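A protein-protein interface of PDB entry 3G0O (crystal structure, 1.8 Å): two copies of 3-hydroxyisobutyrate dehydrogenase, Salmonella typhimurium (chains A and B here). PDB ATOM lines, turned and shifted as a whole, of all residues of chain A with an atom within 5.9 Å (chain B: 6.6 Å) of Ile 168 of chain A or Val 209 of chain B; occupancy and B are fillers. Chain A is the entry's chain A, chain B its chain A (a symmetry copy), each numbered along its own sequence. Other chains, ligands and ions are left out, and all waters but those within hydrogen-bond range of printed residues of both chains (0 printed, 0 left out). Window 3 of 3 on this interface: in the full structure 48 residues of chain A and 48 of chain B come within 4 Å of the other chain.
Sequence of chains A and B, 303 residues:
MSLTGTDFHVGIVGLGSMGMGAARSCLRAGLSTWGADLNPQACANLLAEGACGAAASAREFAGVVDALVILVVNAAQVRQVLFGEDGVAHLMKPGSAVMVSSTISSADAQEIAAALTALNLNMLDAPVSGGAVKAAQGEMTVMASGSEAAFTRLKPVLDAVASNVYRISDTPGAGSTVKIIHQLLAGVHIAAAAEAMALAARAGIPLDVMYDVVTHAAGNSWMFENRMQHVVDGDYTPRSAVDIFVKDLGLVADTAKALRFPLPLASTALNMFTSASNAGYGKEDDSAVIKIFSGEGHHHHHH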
ATOM      1  N   MET A 143     -26.527 -23.050 -10.577  1.00  0.00           N
ATOM      2  CA  MET A 143     -26.506 -22.866  -9.133  1.00  0.00           C
ATOM      3  C   MET A 143     -25.138 -22.243  -8.880  1.00  0.00           C
ATOM      4  O   MET A 143     -24.134 -22.934  -8.702  1.00  0.00           O
ATOM      5  CB  MET A 143     -26.687 -24.208  -8.408  1.00  0.00           C
ATOM      6  CG  MET A 143     -25.965 -25.395  -9.015  1.00  0.00           C
ATOM      7  SD  MET A 143     -27.061 -27.021  -8.926  1.00  0.00           S
ATOM      8  CE  MET A 143     -27.597 -27.074 -10.780  1.00  0.00           C
ATOM      9  N   ALA A 144     -25.114 -20.915  -8.874  1.00  0.00           N
ATOM     10  CA  ALA A 144     -23.869 -20.181  -8.733  1.00  0.00           C
ATOM     11  C   ALA A 144     -23.682 -19.331  -7.495  1.00  0.00           C
ATOM     12  O   ALA A 144     -24.637 -18.839  -6.898  1.00  0.00           O
ATOM     13  CB  ALA A 144     -23.669 -19.311  -9.974  1.00  0.00           C
ATOM     14  N   SER A 145     -22.417 -19.160  -7.129  1.00  0.00           N
ATOM     15  CA  SER A 145     -22.043 -18.331  -5.996  1.00  0.00           C
ATOM     16  C   SER A 145     -20.719 -17.667  -6.367  1.00  0.00           C
ATOM     17  O   SER A 145     -19.866 -18.278  -7.015  1.00  0.00           O
ATOM     18  CB  SER A 145     -21.890 -19.174  -4.722  1.00  0.00           C
ATOM     19  OG  SER A 145     -20.823 -20.095  -4.828  1.00  0.00           O
ATOM     20  N   PHE A 151     -20.303 -12.189 -11.387  1.00  0.00           N
ATOM     21  CA  PHE A 151     -21.660 -12.231 -11.920  1.00  0.00           C
ATOM     22  C   PHE A 151     -21.862 -11.203 -13.024  1.00  0.00           C
ATOM     23  O   PHE A 151     -22.472 -11.492 -14.055  1.00  0.00           O
ATOM     24  CB  PHE A 151     -22.683 -11.981 -10.805  1.00  0.00           C
ATOM     25  CG  PHE A 151     -23.079 -13.225 -10.052  1.00  0.00           C
ATOM     26  CD1 PHE A 151     -23.850 -14.208 -10.667  1.00  0.00           C
ATOM     27  CD2 PHE A 151     -22.665 -13.424  -8.740  1.00  0.00           C
ATOM     28  CE1 PHE A 151     -24.202 -15.375  -9.984  1.00  0.00           C
ATOM     29  CE2 PHE A 151     -23.013 -14.590  -8.050  1.00  0.00           C
ATOM     30  CZ  PHE A 151     -23.782 -15.565  -8.676  1.00  0.00           C
ATOM     31  N   TYR A 166     -29.593 -19.315 -10.206  1.00  0.00           N
ATOM     32  CA  TYR A 166     -29.820 -19.152  -8.778  1.00  0.00           C
ATOM     33  C   TYR A 166     -28.526 -18.704  -8.112  1.00  0.00           C
ATOM     34  O   TYR A 166     -27.540 -19.439  -8.097  1.00  0.00           O
ATOM     35  CB  TYR A 166     -30.302 -20.478  -8.172  1.00  0.00           C
ATOM     36  CG  TYR A 166     -31.614 -20.944  -8.757  1.00  0.00           C
ATOM     37  CD1 TYR A 166     -32.825 -20.393  -8.336  1.00  0.00           C
ATOM     38  CD2 TYR A 166     -31.645 -21.879  -9.790  1.00  0.00           C
ATOM     39  CE1 TYR A 166     -34.028 -20.755  -8.934  1.00  0.00           C
ATOM     40  CE2 TYR A 166     -32.846 -22.246 -10.397  1.00  0.00           C
ATOM     41  CZ  TYR A 166     -34.030 -21.679  -9.965  1.00  0.00           C
ATOM     42  OH  TYR A 166     -35.212 -22.016 -10.579  1.00  0.00           O
ATOM     43  N   ARG A 167     -28.529 -17.483  -7.585  1.00  0.00           N
ATOM     44  CA  ARG A 167     -27.360 -16.933  -6.905  1.00  0.00           C
ATOM     45  C   ARG A 167     -27.462 -17.378  -5.456  1.00  0.00           C
ATOM     46  O   ARG A 167     -28.225 -16.810  -4.667  1.00  0.00           O
ATOM     47  CB  ARG A 167     -27.355 -15.401  -7.007  1.00  0.00           C
ATOM     48  CG  ARG A 167     -27.304 -14.905  -8.448  1.00  0.00           C
ATOM     49  CD  ARG A 167     -27.358 -13.381  -8.570  1.00  0.00           C
ATOM     50  NE  ARG A 167     -26.222 -12.713  -7.935  1.00  0.00           N
ATOM     51  CZ  ARG A 167     -25.773 -11.510  -8.287  1.00  0.00           C
ATOM     52  NH1 ARG A 167     -26.363 -10.846  -9.273  1.00  0.00           N
ATOM     53  NH2 ARG A 167     -24.739 -10.968  -7.653  1.00  0.00           N
ATOM     54  N   ILE A 168     -26.694 -18.412  -5.127  1.00  0.00           N
ATOM     55  CA  ILE A 168     -26.691 -19.004  -3.795  1.00  0.00           C
ATOM     56  C   ILE A 168     -26.022 -18.120  -2.750  1.00  0.00           C
ATOM     57  O   ILE A 168     -26.569 -17.905  -1.669  1.00  0.00           O
ATOM     58  CB  ILE A 168     -25.991 -20.382  -3.820  1.00  0.00           C
ATOM     59  CG1 ILE A 168     -26.513 -21.209  -5.002  1.00  0.00           C
ATOM     60  CG2 ILE A 168     -26.229 -21.113  -2.506  1.00  0.00           C
ATOM     61  CD1 ILE A 168     -28.016 -21.420  -5.012  1.00  0.00           C
ATOM     62  N   SER A 169     -24.833 -17.620  -3.067  1.00  0.00           N
ATOM     63  CA  SER A 169     -24.111 -16.742  -2.149  1.00  0.00           C
ATOM     64  C   SER A 169     -23.188 -15.835  -2.939  1.00  0.00           C
ATOM     65  O   SER A 169     -23.110 -15.927  -4.169  1.00  0.00           O
ATOM     66  CB  SER A 169     -23.291 -17.548  -1.134  1.00  0.00           C
ATOM     67  OG  SER A 169     -22.116 -18.084  -1.717  1.00  0.00           O
ATOM     68  N   ASP A 170     -22.486 -14.960  -2.229  1.00  0.00           N
ATOM     69  CA  ASP A 170     -21.568 -14.027  -2.866  1.00  0.00           C
ATOM     70  C   ASP A 170     -20.137 -14.546  -2.814  1.00  0.00           C
ATOM     71  O   ASP A 170     -19.196 -13.831  -3.148  1.00  0.00           O
ATOM     72  CB  ASP A 170     -21.659 -12.662  -2.177  1.00  0.00           C
ATOM     73  CG  ASP A 170     -21.130 -12.690  -0.757  1.00  0.00           C
ATOM     74  OD1 ASP A 170     -21.330 -13.709  -0.057  1.00  0.00           O
ATOM     75  OD2 ASP A 170     -20.519 -11.687  -0.335  1.00  0.00           O
ATOM     76  N   ALA A 174     -20.567 -22.216  -2.172  1.00  0.00           N
ATOM     77  CA  ALA A 174     -21.974 -22.529  -1.959  1.00  0.00           C
ATOM     78  C   ALA A 174     -22.616 -23.158  -3.189  1.00  0.00           C
ATOM     79  O   ALA A 174     -23.444 -24.061  -3.073  1.00  0.00           O
ATOM     80  CB  ALA A 174     -22.733 -21.277  -1.555  1.00  0.00           C
ATOM     81  N   GLY A 175     -22.237 -22.672  -4.366  1.00  0.00           N
ATOM     82  CA  GLY A 175     -22.783 -23.222  -5.587  1.00  0.00           C
ATOM     83  C   GLY A 175     -22.471 -24.705  -5.693  1.00  0.00           C
ATOM     84  O   GLY A 175     -23.351 -25.504  -6.010  1.00  0.00           O
ATOM     85  N   VAL A 178     -24.565 -26.863  -3.403  1.00  0.00           N
ATOM     86  CA  VAL A 178     -25.910 -27.092  -3.915  1.00  0.00           C
ATOM     87  C   VAL A 178     -25.890 -28.183  -4.978  1.00  0.00           C
ATOM     88  O   VAL A 178     -26.785 -29.029  -5.018  1.00  0.00           O
ATOM     89  CB  VAL A 178     -26.506 -25.800  -4.504  1.00  0.00           C
ATOM     90  CG1 VAL A 178     -27.813 -26.100  -5.235  1.00  0.00           C
ATOM     91  CG2 VAL A 178     -26.753 -24.799  -3.384  1.00  0.00           C
ATOM     92  N   ILE B 205     -28.101 -24.616   3.566  1.00  0.00           N
ATOM     93  CA  ILE B 205     -28.691 -24.105   2.336  1.00  0.00           C
ATOM     94  C   ILE B 205     -30.176 -23.838   2.585  1.00  0.00           C
ATOM     95  O   ILE B 205     -30.888 -24.714   3.073  1.00  0.00           O
ATOM     96  CB  ILE B 205     -28.585 -25.129   1.175  1.00  0.00           C
ATOM     97  CG1 ILE B 205     -27.122 -25.514   0.931  1.00  0.00           C
ATOM     98  CG2 ILE B 205     -29.223 -24.551  -0.088  1.00  0.00           C
ATOM     99  CD1 ILE B 205     -26.221 -24.346   0.555  1.00  0.00           C
ATOM    100  N   PRO B 206     -30.658 -22.621   2.270  1.00  0.00           N
ATOM    101  CA  PRO B 206     -32.079 -22.324   2.485  1.00  0.00           C
ATOM    102  C   PRO B 206     -32.917 -23.356   1.725  1.00  0.00           C
ATOM    103  O   PRO B 206     -32.650 -23.634   0.556  1.00  0.00           O
ATOM    104  CB  PRO B 206     -32.225 -20.914   1.910  1.00  0.00           C
ATOM    105  CG  PRO B 206     -30.881 -20.306   2.177  1.00  0.00           C
ATOM    106  CD  PRO B 206     -29.942 -21.427   1.780  1.00  0.00           C
ATOM    107  N   LEU B 207     -33.926 -23.919   2.383  1.00  0.00           N
ATOM    108  CA  LEU B 207     -34.760 -24.939   1.752  1.00  0.00           C
ATOM    109  C   LEU B 207     -35.582 -24.440   0.568  1.00  0.00           C
ATOM    110  O   LEU B 207     -35.796 -25.182  -0.395  1.00  0.00           O
ATOM    111  CB  LEU B 207     -35.680 -25.589   2.789  1.00  0.00           C
ATOM    112  CG  LEU B 207     -34.976 -26.317   3.941  1.00  0.00           C
ATOM    113  CD1 LEU B 207     -36.004 -27.098   4.746  1.00  0.00           C
ATOM    114  CD2 LEU B 207     -33.913 -27.251   3.394  1.00  0.00           C
ATOM    115  N   ASP B 208     -36.042 -23.192   0.626  1.00  0.00           N
ATOM    116  CA  ASP B 208     -36.829 -22.662  -0.480  1.00  0.00           C
ATOM    117  C   ASP B 208     -35.931 -22.566  -1.718  1.00  0.00           C
ATOM    118  O   ASP B 208     -36.357 -22.879  -2.831  1.00  0.00           O
ATOM    119  CB  ASP B 208     -37.457 -21.303  -0.100  1.00  0.00           C
ATOM    120  CG  ASP B 208     -36.426 -20.227   0.225  1.00  0.00           C
ATOM    121  OD1 ASP B 208     -35.339 -20.540   0.750  1.00  0.00           O
ATOM    122  OD2 ASP B 208     -36.728 -19.045  -0.030  1.00  0.00           O
ATOM    123  N   VAL B 209     -34.678 -22.172  -1.507  1.00  0.00           N
ATOM    124  CA  VAL B 209     -33.708 -22.067  -2.594  1.00  0.00           C
ATOM    125  C   VAL B 209     -33.390 -23.461  -3.143  1.00  0.00           C
ATOM    126  O   VAL B 209     -33.333 -23.668  -4.352  1.00  0.00           O
ATOM    127  CB  VAL B 209     -32.391 -21.419  -2.112  1.00  0.00           C
ATOM    128  CG1 VAL B 209     -31.366 -21.427  -3.233  1.00  0.00           C
ATOM    129  CG2 VAL B 209     -32.655 -19.993  -1.636  1.00  0.00           C
ATOM    130  N   MET B 210     -33.177 -24.414  -2.241  1.00  0.00           N
ATOM    131  CA  MET B 210     -32.870 -25.773  -2.663  1.00  0.00           C
ATOM    132  C   MET B 210     -34.044 -26.331  -3.464  1.00  0.00           C
ATOM    133  O   MET B 210     -33.851 -27.014  -4.472  1.00  0.00           O
ATOM    134  CB  MET B 210     -32.581 -26.665  -1.452  1.00  0.00           C
ATOM    135  CG  MET B 210     -31.912 -28.000  -1.798  1.00  0.00           C
ATOM    136  SD  MET B 210     -30.085 -27.799  -2.466  1.00  0.00           S
ATOM    137  CE  MET B 210     -30.199 -28.843  -4.100  1.00  0.00           C
ATOM    138  N   TYR B 211     -35.260 -26.023  -3.020  1.00  0.00           N
ATOM    139  CA  TYR B 211     -36.467 -26.486  -3.697  1.00  0.00           C
ATOM    140  C   TYR B 211     -36.545 -25.952  -5.129  1.00  0.00           C
ATOM    141  O   TYR B 211     -36.780 -26.711  -6.067  1.00  0.00           O
ATOM    142  CB  TYR B 211     -37.712 -26.041  -2.929  1.00  0.00           C
ATOM    143  CG  TYR B 211     -39.007 -26.490  -3.571  1.00  0.00           C
ATOM    144  CD1 TYR B 211     -39.528 -27.759  -3.329  1.00  0.00           C
ATOM    145  CD2 TYR B 211     -39.712 -25.639  -4.423  1.00  0.00           C
ATOM    146  CE1 TYR B 211     -40.720 -28.168  -3.915  1.00  0.00           C
ATOM    147  CE2 TYR B 211     -40.898 -26.038  -5.014  1.00  0.00           C
ATOM    148  CZ  TYR B 211     -41.399 -27.301  -4.754  1.00  0.00           C
ATOM    149  OH  TYR B 211     -42.585 -27.690  -5.325  1.00  0.00           O
ATOM    150  N   ASP B 212     -36.347 -24.646  -5.293  1.00  0.00           N
ATOM    151  CA  ASP B 212     -36.402 -24.041  -6.623  1.00  0.00           C
ATOM    152  C   ASP B 212     -35.372 -24.640  -7.572  1.00  0.00           C
ATOM    153  O   ASP B 212     -35.672 -24.901  -8.730  1.00  0.00           O
ATOM    154  CB  ASP B 212     -36.196 -22.523  -6.545  1.00  0.00           C
ATOM    155  CG  ASP B 212     -37.332 -21.815  -5.838  1.00  0.00           C
ATOM    156  OD1 ASP B 212     -38.486 -22.285  -5.943  1.00  0.00           O
ATOM    157  OD2 ASP B 212     -37.077 -20.781  -5.187  1.00  0.00           O
ATOM    158  N   VAL B 213     -34.155 -24.854  -7.081  1.00  0.00           N
ATOM    159  CA  VAL B 213     -33.103 -25.422  -7.916  1.00  0.00           C
ATOM    160  C   VAL B 213     -33.487 -26.815  -8.394  1.00  0.00           C
ATOM    161  O   VAL B 213     -33.490 -27.088  -9.594  1.00  0.00           O
ATOM    162  CB  VAL B 213     -31.761 -25.516  -7.149  1.00  0.00           C
ATOM    163  CG1 VAL B 213     -30.758 -26.371  -7.926  1.00  0.00           C
ATOM    164  CG2 VAL B 213     -31.202 -24.125  -6.903  1.00  0.00           C
ATOM    165  N   VAL B 214     -33.815 -27.698  -7.456  1.00  0.00           N
ATOM    166  CA  VAL B 214     -34.173 -29.058  -7.824  1.00  0.00           C
ATOM    167  C   VAL B 214     -35.342 -29.121  -8.799  1.00  0.00           C
ATOM    168  O   VAL B 214     -35.282 -29.837  -9.798  1.00  0.00           O
ATOM    169  CB  VAL B 214     -34.520 -29.915  -6.587  1.00  0.00           C
ATOM    170  CG1 VAL B 214     -35.040 -31.276  -7.033  1.00  0.00           C
ATOM    171  CG2 VAL B 214     -33.286 -30.085  -5.707  1.00  0.00           C
ATOM    172  N   VAL B 232     -40.993 -27.086   2.916  1.00  0.00           N
ATOM    173  CA  VAL B 232     -40.607 -25.685   2.846  1.00  0.00           C
ATOM    174  C   VAL B 232     -41.583 -24.841   3.659  1.00  0.00           C
ATOM    175  O   VAL B 232     -41.179 -23.903   4.351  1.00  0.00           O
ATOM    176  CB  VAL B 232     -40.596 -25.178   1.388  1.00  0.00           C
ATOM    177  CG1 VAL B 232     -40.307 -23.687   1.359  1.00  0.00           C
ATOM    178  CG2 VAL B 232     -39.540 -25.933   0.584  1.00  0.00           C
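Among the printed residues, pairs that only touch across the chains: Val 178 of chain A with Met 210 of chain B (3.5 Å), Tyr 166 of chain A with Val 213 of chain B (3.7 Å), Ile 168 of chain A with Val 209 of chain B (3.8 Å), Met 143 of chain A with Val 213 of chain B (3.9 Å) and Val 178 of chain A with Val 213 of chain B (3.998 Å).
Hydrophobic or aromatic side chains of chain B within 4 Å of the printed part of chain A: Val 209, Met 210 and Val 213. Of the 12 printed residues of chain A, 4 touch a printed residue of chain B. Hydrophobic or aromatic side chains of chain A within 4 Å of the printed part of chain B: Met 143, Tyr 166, Ile 168 and Val 178. Among the printed residues, 6 pairs touch across the chains. Among the printed residues, no Asp or Glu carboxylate lies within 4 Å of a Lys or Arg side-chain nitrogen of the other chain.
The backbone NH (N) of Ala 144 of chain A lies within hydrogen-bond range of the backbone carbonyl oxygen (O) of Tyr 166 of chain A (2.9 Å). The backbone carbonyl oxygen of Ala 144 of chain A sits at hydrogen-bond distance from the backbone NH of Ile 168 of chain A (2.7 Å).
No position is printed for both chains. Of the 6 pairs that touch across the chains among the printed residues, none has its exchanged pair printed and touching as well.
Of the printed residues of chain B, Met 143 of chain A touches Val 213. Of the printed residues of chain B, Tyr 166 of chain A touches Asp 212 (3.5 Å) and Val 213 (3.7 Å). Of chain B, only Val 209 (3.8 Å) comes within 4 Å of Ile 168 of chain A. Ser 169 of chain A touches none of the printed residues of chain B. Of the printed residues of chain A, Val 209 of chain B touches Ile 168 (3.8 Å). Of the printed residues of chain A, Met 210 of chain B touches Val 178. Printed residues of chain A within 4 Å of Asp 212 of chain B: Tyr 166 (3.5 Å). Of the printed residues of chain A, Val 213 of chain B touches Met 143 (3.9 Å), Tyr 166 (3.7 Å) and Val 178 (3.998 Å). Val 232 of chain B touches none of the printed residues of chain A. The nearest printed residue of chain B that does not touch Tyr 166 of chain A is Val 209 of chain B (5.1 Å).
OH of Tyr 166 of chain A sits at hydrogen-bond distance from O of Asp 212 of chain B.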
